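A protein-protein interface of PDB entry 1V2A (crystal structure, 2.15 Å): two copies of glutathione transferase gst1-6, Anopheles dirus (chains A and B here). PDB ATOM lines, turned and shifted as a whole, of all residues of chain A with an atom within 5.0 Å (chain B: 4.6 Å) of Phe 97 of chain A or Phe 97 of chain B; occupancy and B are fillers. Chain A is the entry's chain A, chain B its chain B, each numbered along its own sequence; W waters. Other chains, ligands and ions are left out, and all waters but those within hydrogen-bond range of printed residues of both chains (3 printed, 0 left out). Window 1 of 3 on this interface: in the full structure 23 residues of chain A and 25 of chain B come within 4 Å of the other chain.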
ATOM      1  N   GLU A  63       6.010  26.811  -2.499  1.00  0.00           N
ATOM      2  CA  GLU A  63       7.086  26.208  -3.280  1.00  0.00           C
ATOM      3  C   GLU A  63       8.321  26.623  -2.461  1.00  0.00           C
ATOM      4  O   GLU A  63       8.692  27.804  -2.431  1.00  0.00           O
ATOM      5  CB  GLU A  63       7.197  26.791  -4.694  1.00  0.00           C
ATOM      6  CG  GLU A  63       6.305  26.150  -5.753  1.00  0.00           C
ATOM      7  CD  GLU A  63       6.644  24.698  -6.022  1.00  0.00           C
ATOM      8  OE1 GLU A  63       7.838  24.338  -5.978  1.00  0.00           O
ATOM      9  OE2 GLU A  63       5.717  23.906  -6.292  1.00  0.00           O
ATOM     10  N   TYR A  65      11.424  26.686  -2.871  1.00  0.00           N
ATOM     11  CA  TYR A  65      12.346  27.567  -3.571  1.00  0.00           C
ATOM     12  C   TYR A  65      11.865  29.019  -3.628  1.00  0.00           C
ATOM     13  O   TYR A  65      12.669  29.948  -3.540  1.00  0.00           O
ATOM     14  CB  TYR A  65      12.607  27.034  -4.982  1.00  0.00           C
ATOM     15  CG  TYR A  65      12.951  25.558  -5.013  1.00  0.00           C
ATOM     16  CD1 TYR A  65      11.950  24.591  -5.084  1.00  0.00           C
ATOM     17  CD2 TYR A  65      14.273  25.129  -4.923  1.00  0.00           C
ATOM     18  CE1 TYR A  65      12.258  23.230  -5.059  1.00  0.00           C
ATOM     19  CE2 TYR A  65      14.591  23.769  -4.900  1.00  0.00           C
ATOM     20  CZ  TYR A  65      13.580  22.827  -4.969  1.00  0.00           C
ATOM     21  OH  TYR A  65      13.889  21.483  -4.959  1.00  0.00           O
ATOM     22  N   ALA A  66      10.558  29.223  -3.767  1.00  0.00           N
ATOM     23  CA  ALA A  66      10.026  30.583  -3.829  1.00  0.00           C
ATOM     24  C   ALA A  66       9.987  31.195  -2.435  1.00  0.00           C
ATOM     25  O   ALA A  66      10.088  32.404  -2.273  1.00  0.00           O
ATOM     26  CB  ALA A  66       8.637  30.573  -4.438  1.00  0.00           C
ATOM     27  N   ASN A  93      20.655  29.559  -9.620  1.00  0.00           N
ATOM     28  CA  ASN A  93      19.381  29.236 -10.252  1.00  0.00           C
ATOM     29  C   ASN A  93      19.428  27.876 -10.914  1.00  0.00           C
ATOM     30  O   ASN A  93      18.546  27.050 -10.688  1.00  0.00           O
ATOM     31  CB  ASN A  93      18.992  30.294 -11.280  1.00  0.00           C
ATOM     32  CG  ASN A  93      18.489  31.558 -10.631  1.00  0.00           C
ATOM     33  OD1 ASN A  93      18.122  31.543  -9.461  1.00  0.00           O
ATOM     34  ND2 ASN A  93      18.457  32.658 -11.383  1.00  0.00           N
ATOM     35  N   GLN A  94      20.457  27.650 -11.728  1.00  0.00           N
ATOM     36  CA  GLN A  94      20.600  26.377 -12.401  1.00  0.00           C
ATOM     37  C   GLN A  94      20.539  25.263 -11.369  1.00  0.00           C
ATOM     38  O   GLN A  94      19.849  24.271 -11.583  1.00  0.00           O
ATOM     39  CB  GLN A  94      21.928  26.310 -13.172  1.00  0.00           C
ATOM     40  CG  GLN A  94      22.131  25.032 -13.994  1.00  0.00           C
ATOM     41  CD  GLN A  94      22.977  23.993 -13.280  1.00  0.00           C
ATOM     42  OE1 GLN A  94      22.560  22.852 -13.099  1.00  0.00           O
ATOM     43  NE2 GLN A  94      24.175  24.382 -12.879  1.00  0.00           N
ATOM     44  N   ARG A  95      21.249  25.426 -10.252  1.00  0.00           N
ATOM     45  CA  ARG A  95      21.255  24.407  -9.202  1.00  0.00           C
ATOM     46  C   ARG A  95      19.882  24.265  -8.529  1.00  0.00           C
ATOM     47  O   ARG A  95      19.501  23.168  -8.122  1.00  0.00           O
ATOM     48  CB  ARG A  95      22.287  24.719  -8.111  1.00  0.00           C
ATOM     49  CG  ARG A  95      23.684  25.131  -8.570  1.00  0.00           C
ATOM     50  CD  ARG A  95      24.368  24.162  -9.519  1.00  0.00           C
ATOM     51  NE  ARG A  95      25.815  24.190  -9.311  1.00  0.00           N
ATOM     52  CZ  ARG A  95      26.732  23.953 -10.246  1.00  0.00           C
ATOM     53  NH1 ARG A  95      26.373  23.669 -11.494  1.00  0.00           N
ATOM     54  NH2 ARG A  95      28.017  23.983  -9.922  1.00  0.00           N
ATOM     55  N   LEU A  96      19.147  25.367  -8.400  1.00  0.00           N
ATOM     56  CA  LEU A  96      17.835  25.298  -7.774  1.00  0.00           C
ATOM     57  C   LEU A  96      16.876  24.510  -8.644  1.00  0.00           C
ATOM     58  O   LEU A  96      16.123  23.674  -8.143  1.00  0.00           O
ATOM     59  CB  LEU A  96      17.262  26.698  -7.524  1.00  0.00           C
ATOM     60  CG  LEU A  96      17.909  27.572  -6.453  1.00  0.00           C
ATOM     61  CD1 LEU A  96      17.161  28.896  -6.380  1.00  0.00           C
ATOM     62  CD2 LEU A  96      17.886  26.854  -5.101  1.00  0.00           C
ATOM     63  N   PHE A  97      16.889  24.783  -9.947  1.00  0.00           N
ATOM     64  CA  PHE A  97      16.014  24.067 -10.863  1.00  0.00           C
ATOM     65  C   PHE A  97      16.532  22.655 -11.098  1.00  0.00           C
ATOM     66  O   PHE A  97      15.789  21.772 -11.525  1.00  0.00           O
ATOM     67  CB  PHE A  97      15.855  24.838 -12.175  1.00  0.00           C
ATOM     68  CG  PHE A  97      14.945  26.030 -12.054  1.00  0.00           C
ATOM     69  CD1 PHE A  97      15.456  27.291 -11.776  1.00  0.00           C
ATOM     70  CD2 PHE A  97      13.565  25.871 -12.150  1.00  0.00           C
ATOM     71  CE1 PHE A  97      14.611  28.369 -11.595  1.00  0.00           C
ATOM     72  CE2 PHE A  97      12.709  26.943 -11.969  1.00  0.00           C
ATOM     73  CZ  PHE A  97      13.230  28.197 -11.690  1.00  0.00           C
ATOM     74  N   PHE A  98      17.804  22.448 -10.790  1.00  0.00           N
ATOM     75  CA  PHE A  98      18.430  21.134 -10.888  1.00  0.00           C
ATOM     76  C   PHE A  98      17.889  20.329  -9.709  1.00  0.00           C
ATOM     77  O   PHE A  98      17.574  19.150  -9.820  1.00  0.00           O
ATOM     78  CB  PHE A  98      19.946  21.271 -10.740  1.00  0.00           C
ATOM     79  CG  PHE A  98      20.645  19.989 -10.389  1.00  0.00           C
ATOM     80  CD1 PHE A  98      20.859  19.009 -11.350  1.00  0.00           C
ATOM     81  CD2 PHE A  98      21.080  19.756  -9.086  1.00  0.00           C
ATOM     82  CE1 PHE A  98      21.508  17.808 -11.025  1.00  0.00           C
ATOM     83  CE2 PHE A  98      21.731  18.559  -8.748  1.00  0.00           C
ATOM     84  CZ  PHE A  98      21.942  17.581  -9.721  1.00  0.00           C
ATOM     85  N   ASP A  99      17.785  21.003  -8.569  1.00  0.00           N
ATOM     86  CA  ASP A  99      17.302  20.396  -7.343  1.00  0.00           C
ATOM     87  C   ASP A  99      15.878  19.867  -7.490  1.00  0.00           C
ATOM     88  O   ASP A  99      15.619  18.698  -7.234  1.00  0.00           O
ATOM     89  CB  ASP A  99      17.378  21.425  -6.208  1.00  0.00           C
ATOM     90  CG  ASP A  99      17.025  20.842  -4.847  1.00  0.00           C
ATOM     91  OD1 ASP A  99      17.522  19.744  -4.508  1.00  0.00           O
ATOM     92  OD2 ASP A  99      16.269  21.497  -4.105  1.00  0.00           O
ATOM     93  N   ILE A 100      14.956  20.718  -7.918  1.00  0.00           N
ATOM     94  CA  ILE A 100      13.562  20.303  -8.044  1.00  0.00           C
ATOM     95  C   ILE A 100      13.247  19.439  -9.253  1.00  0.00           C
ATOM     96  O   ILE A 100      12.407  18.541  -9.160  1.00  0.00           O
ATOM     97  CB  ILE A 100      12.603  21.528  -8.081  1.00  0.00           C
ATOM     98  CG1 ILE A 100      11.143  21.060  -8.002  1.00  0.00           C
ATOM     99  CG2 ILE A 100      12.825  22.325  -9.358  1.00  0.00           C
ATOM    100  CD1 ILE A 100      10.107  22.192  -8.176  1.00  0.00           C
ATOM    101  N   GLY A 101      13.914  19.700 -10.376  1.00  0.00           N
ATOM    102  CA  GLY A 101      13.632  18.949 -11.590  1.00  0.00           C
ATOM    103  C   GLY A 101      14.482  17.727 -11.905  1.00  0.00           C
ATOM    104  O   GLY A 101      14.137  16.929 -12.782  1.00  0.00           O
ATOM    105  N   THR A 102      15.589  17.565 -11.201  1.00  0.00           N
ATOM    106  CA  THR A 102      16.453  16.426 -11.463  1.00  0.00           C
ATOM    107  C   THR A 102      16.793  15.631 -10.202  1.00  0.00           C
ATOM    108  O   THR A 102      16.268  14.529  -9.980  1.00  0.00           O
ATOM    109  CB  THR A 102      17.771  16.875 -12.128  1.00  0.00           C
ATOM    110  OG1 THR A 102      17.482  17.673 -13.285  1.00  0.00           O
ATOM    111  CG2 THR A 102      18.585  15.675 -12.553  1.00  0.00           C
ATOM    112  N   GLU B  63      19.269  25.067 -18.210  1.00  0.00           N
ATOM    113  CA  GLU B  63      17.973  25.002 -17.542  1.00  0.00           C
ATOM    114  C   GLU B  63      17.294  26.235 -18.121  1.00  0.00           C
ATOM    115  O   GLU B  63      17.653  27.367 -17.779  1.00  0.00           O
ATOM    116  CB  GLU B  63      18.056  25.164 -16.013  1.00  0.00           C
ATOM    117  CG  GLU B  63      18.416  23.922 -15.196  1.00  0.00           C
ATOM    118  CD  GLU B  63      17.430  22.777 -15.360  1.00  0.00           C
ATOM    119  OE1 GLU B  63      16.202  23.014 -15.396  1.00  0.00           O
ATOM    120  OE2 GLU B  63      17.896  21.627 -15.437  1.00  0.00           O
ATOM    121  N   TYR B  65      14.984  27.850 -17.471  1.00  0.00           N
ATOM    122  CA  TYR B  65      14.613  28.843 -16.476  1.00  0.00           C
ATOM    123  C   TYR B  65      15.797  29.692 -16.040  1.00  0.00           C
ATOM    124  O   TYR B  65      15.658  30.893 -15.828  1.00  0.00           O
ATOM    125  CB  TYR B  65      13.995  28.151 -15.266  1.00  0.00           C
ATOM    126  CG  TYR B  65      12.905  27.188 -15.646  1.00  0.00           C
ATOM    127  CD1 TYR B  65      13.199  25.874 -15.981  1.00  0.00           C
ATOM    128  CD2 TYR B  65      11.577  27.599 -15.703  1.00  0.00           C
ATOM    129  CE1 TYR B  65      12.191  24.986 -16.366  1.00  0.00           C
ATOM    130  CE2 TYR B  65      10.559  26.715 -16.089  1.00  0.00           C
ATOM    131  CZ  TYR B  65      10.878  25.415 -16.421  1.00  0.00           C
ATOM    132  OH  TYR B  65       9.896  24.559 -16.855  1.00  0.00           O
ATOM    133  N   ASN B  93       8.235  33.547  -9.422  1.00  0.00           N
ATOM    134  CA  ASN B  93       9.092  32.432  -9.035  1.00  0.00           C
ATOM    135  C   ASN B  93       8.286  31.185  -8.744  1.00  0.00           C
ATOM    136  O   ASN B  93       8.636  30.098  -9.205  1.00  0.00           O
ATOM    137  CB  ASN B  93       9.927  32.778  -7.807  1.00  0.00           C
ATOM    138  CG  ASN B  93      11.153  33.582  -8.159  1.00  0.00           C
ATOM    139  OD1 ASN B  93      11.518  33.692  -9.329  1.00  0.00           O
ATOM    140  ND2 ASN B  93      11.803  34.136  -7.151  1.00  0.00           N
ATOM    141  N   GLN B  94       7.206  31.337  -7.980  1.00  0.00           N
ATOM    142  CA  GLN B  94       6.370  30.193  -7.646  1.00  0.00           C
ATOM    143  C   GLN B  94       5.766  29.566  -8.898  1.00  0.00           C
ATOM    144  O   GLN B  94       5.774  28.342  -9.042  1.00  0.00           O
ATOM    145  CB  GLN B  94       5.264  30.598  -6.675  1.00  0.00           C
ATOM    146  CG  GLN B  94       4.301  29.467  -6.342  1.00  0.00           C
ATOM    147  CD  GLN B  94       3.151  29.371  -7.324  1.00  0.00           C
ATOM    148  OE1 GLN B  94       2.941  28.337  -7.963  1.00  0.00           O
ATOM    149  NE2 GLN B  94       2.395  30.461  -7.451  1.00  0.00           N
ATOM    150  N   ARG B  95       5.256  30.399  -9.806  1.00  0.00           N
ATOM    151  CA  ARG B  95       4.659  29.890 -11.036  1.00  0.00           C
ATOM    152  C   ARG B  95       5.710  29.173 -11.892  1.00  0.00           C
ATOM    153  O   ARG B  95       5.382  28.247 -12.642  1.00  0.00           O
ATOM    154  CB  ARG B  95       4.037  31.019 -11.865  1.00  0.00           C
ATOM    155  CG  ARG B  95       3.086  31.965 -11.136  1.00  0.00           C
ATOM    156  CD  ARG B  95       1.835  31.308 -10.584  1.00  0.00           C
ATOM    157  NE  ARG B  95       0.715  32.246 -10.577  1.00  0.00           N
ATOM    158  CZ  ARG B  95      -0.270  32.249  -9.682  1.00  0.00           C
ATOM    159  NH1 ARG B  95      -0.285  31.362  -8.694  1.00  0.00           N
ATOM    160  NH2 ARG B  95      -1.253  33.132  -9.784  1.00  0.00           N
ATOM    161  N   LEU B  96       6.968  29.611 -11.798  1.00  0.00           N
ATOM    162  CA  LEU B  96       8.030  28.978 -12.566  1.00  0.00           C
ATOM    163  C   LEU B  96       8.317  27.583 -12.002  1.00  0.00           C
ATOM    164  O   LEU B  96       8.566  26.648 -12.755  1.00  0.00           O
ATOM    165  CB  LEU B  96       9.317  29.821 -12.539  1.00  0.00           C
ATOM    166  CG  LEU B  96       9.372  31.147 -13.309  1.00  0.00           C
ATOM    167  CD1 LEU B  96      10.688  31.859 -13.009  1.00  0.00           C
ATOM    168  CD2 LEU B  96       9.243  30.903 -14.803  1.00  0.00           C
ATOM    169  N   PHE B  97       8.295  27.444 -10.680  1.00  0.00           N
ATOM    170  CA  PHE B  97       8.541  26.146 -10.070  1.00  0.00           C
ATOM    171  C   PHE B  97       7.329  25.252 -10.233  1.00  0.00           C
ATOM    172  O   PHE B  97       7.419  24.026 -10.147  1.00  0.00           O
ATOM    173  CB  PHE B  97       8.946  26.298  -8.599  1.00  0.00           C
ATOM    174  CG  PHE B  97      10.377  26.740  -8.426  1.00  0.00           C
ATOM    175  CD1 PHE B  97      10.697  28.087  -8.305  1.00  0.00           C
ATOM    176  CD2 PHE B  97      11.410  25.810  -8.458  1.00  0.00           C
ATOM    177  CE1 PHE B  97      12.030  28.509  -8.219  1.00  0.00           C
ATOM    178  CE2 PHE B  97      12.744  26.214  -8.377  1.00  0.00           C
ATOM    179  CZ  PHE B  97      13.056  27.569  -8.257  1.00  0.00           C
ATOM    180  N   PHE B  98       6.198  25.889 -10.500  1.00  0.00           N
ATOM    181  CA  PHE B  98       4.948  25.193 -10.752  1.00  0.00           C
ATOM    182  C   PHE B  98       5.089  24.546 -12.134  1.00  0.00           C
ATOM    183  O   PHE B  98       4.662  23.415 -12.366  1.00  0.00           O
ATOM    184  CB  PHE B  98       3.794  26.201 -10.778  1.00  0.00           C
ATOM    185  CG  PHE B  98       2.551  25.679 -11.434  1.00  0.00           C
ATOM    186  CD1 PHE B  98       1.744  24.750 -10.787  1.00  0.00           C
ATOM    187  CD2 PHE B  98       2.197  26.100 -12.711  1.00  0.00           C
ATOM    188  CE1 PHE B  98       0.602  24.250 -11.405  1.00  0.00           C
ATOM    189  CE2 PHE B  98       1.066  25.610 -13.332  1.00  0.00           C
ATOM    190  CZ  PHE B  98       0.265  24.684 -12.683  1.00  0.00           C
ATOM    191  N   ASP B  99       5.721  25.283 -13.041  1.00  0.00           N
ATOM    192  CA  ASP B  99       5.927  24.833 -14.407  1.00  0.00           C
ATOM    193  C   ASP B  99       6.829  23.621 -14.502  1.00  0.00           C
ATOM    194  O   ASP B  99       6.428  22.566 -15.000  1.00  0.00           O
ATOM    195  CB  ASP B  99       6.527  25.968 -15.238  1.00  0.00           C
ATOM    196  CG  ASP B  99       6.535  25.663 -16.717  1.00  0.00           C
ATOM    197  OD1 ASP B  99       5.464  25.331 -17.257  1.00  0.00           O
ATOM    198  OD2 ASP B  99       7.607  25.757 -17.343  1.00  0.00           O
ATOM    199  N   ILE B 100       8.053  23.768 -14.021  1.00  0.00           N
ATOM    200  CA  ILE B 100       9.003  22.684 -14.103  1.00  0.00           C
ATOM    201  C   ILE B 100       8.627  21.473 -13.266  1.00  0.00           C
ATOM    202  O   ILE B 100       8.789  20.336 -13.724  1.00  0.00           O
ATOM    203  CB  ILE B 100      10.429  23.149 -13.708  1.00  0.00           C
ATOM    204  CG1 ILE B 100      11.431  22.054 -14.062  1.00  0.00           C
ATOM    205  CG2 ILE B 100      10.505  23.466 -12.219  1.00  0.00           C
ATOM    206  CD1 ILE B 100      12.873  22.390 -13.737  1.00  0.00           C
ATOM    207  N   GLY B 101       8.120  21.708 -12.053  1.00  0.00           N
ATOM    208  CA  GLY B 101       7.772  20.609 -11.174  1.00  0.00           C
ATOM    209  C   GLY B 101       6.324  20.155 -11.078  1.00  0.00           C
ATOM    210  O   GLY B 101       6.038  19.160 -10.418  1.00  0.00           O
ATOM    211  N   THR B 102       5.399  20.859 -11.714  1.00  0.00           N
ATOM    212  CA  THR B 102       4.010  20.439 -11.623  1.00  0.00           C
ATOM    213  C   THR B 102       3.364  20.191 -12.970  1.00  0.00           C
ATOM    214  O   THR B 102       3.083  19.048 -13.321  1.00  0.00           O
ATOM    215  CB  THR B 102       3.156  21.471 -10.862  1.00  0.00           C
ATOM    216  OG1 THR B 102       3.666  21.619  -9.531  1.00  0.00           O
ATOM    217  CG2 THR B 102       1.694  21.022 -10.799  1.00  0.00           C
HETATM  218  O   HOH W   1      16.301  20.138 -13.601  1.00  0.00           O
HETATM  219  O   HOH W   2       3.711  25.693  -7.605  1.00  0.00           O
HETATM  220  O   HOH W   3      19.915  21.398 -13.987  1.00  0.00           O
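The side-chain amide nitrogen (NE2) of Gln 94 of chain B lies close to the guanidinium group (NH1) of Arg 95 of chain B.
The side-chain hydroxyl of Tyr 65 of chain A sits at hydrogen-bond distance from the side-chain carboxylate of Asp 99 of chain A, 2.5 Å away.
The side-chain amide nitrogen of Gln 94 of chain A lies close to the guanidinium group of Arg 95 of chain A, at 2.7 Å.
The side-chain hydroxyl of Tyr 65 of chain B is in hydrogen-bond range of the side-chain carboxylate of Asp 99 of chain B, 2.6 Å away.
The backbone NH (N) of Ile 100 of chain B sits close to the side-chain hydroxyl (OH) of Tyr 65 of chain B, 3.5 Å away.
The side-chain hydroxyl of Tyr 65 of chain A is in hydrogen-bond range of the backbone NH of Ile 100 of chain A.
Among the printed residues, pairs that only touch across the chains: Glu 63 of chain A with Gln 94 of chain B (3.9 Å), Glu 63 of chain A with Phe 97 of chain B (3.5 Å), Tyr 65 of chain A with Phe 97 of chain B (3.3 Å), Ala 66 of chain A with Gln 94 of chain B (3.9 Å), Gln 94 of chain A with Glu 63 of chain B (3.9 Å), Phe 97 of chain A with Glu 63 of chain B (3.7 Å), Phe 97 of chain A with Tyr 65 of chain B (3.7 Å), Phe 97 of chain A with Phe 97 of chain B (3.5 Å), Phe 97 of chain A with Ile 100 of chain B (3.7 Å), Ile 100 of chain A with Phe 97 of chain B (3.8 Å) and Ile 100 of chain A with Ile 100 of chain B (3.9 Å).
Of chain B, only Glu 63, Tyr 65, Phe 97 and Ile 100 come within 4 Å of Phe 97 of chain A.
Phe 97 of chain B touches four residues of chain A.
Of the printed residues of chain A, Gln 94 of chain B touches Glu 63 (3.9 Å) and Ala 66 (3.9 Å).
Of the printed residues of chain B, Glu 63 of chain A touches Gln 94 and Phe 97.
Of the printed residues of chain B, Ala 66 of chain A touches Gln 94.
Printed residues of chain A within 4 Å of Ile 100 of chain B: Phe 97 and Ile 100.
Printed residues of chain B within 4 Å of Gln 94 of chain A: Glu 63.
Gly 101 of chain A touches none of the printed residues of chain B.
Arg 95 of chain B touches none of the printed residues of chain A.
The nearest residue of chain A that does not touch Phe 97 of chain B is Leu 96 of chain A (4.2 Å).
Of the 12 printed residues of chain B, 5 touch a printed residue of chain A.
Printed residues of chain B that touch a printed residue of chain A: Glu 63, Tyr 65, Gln 94, Phe 97 and Ile 100.
Among the printed residues, no Asp or Glu carboxylate lies within 4 Å of a Lys or Arg side-chain nitrogen of the other chain.
Glu 63 of chain A touches Phe 97 of chain B, and with the chains exchanged Phe 97 of chain A touches Glu 63 of chain B.
Tyr 65 of chain A touches Phe 97 of chain B, and with the chains exchanged Phe 97 of chain A touches Tyr 65 of chain B.
Phe 97 of chain A touches its own counterpart, Phe 97 of chain B.
Ile 100 of chain B touches its own counterpart, Ile 100 of chain A.
Of the 11 pairs that touch across the chains among the printed residues, 10 have their exchanged pair printed and touching as well.
Water W3 lies within hydrogen-bond range of OE2 of Glu 63 of chain B (2.5 Å) and OE1 of Gln 94 of chain A (3.1 Å).
Water W1 lies within hydrogen-bond range of O of Phe 97 of chain A, OG1 of Thr 102 of chain A and OE2 of Glu 63 of chain B.
Water W2 lies within hydrogen-bond range of the side-chain amide oxygen of Gln 94 of chain B (2.8 Å) and the side-chain carboxylate of Glu 63 of chain A (3.0 Å).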
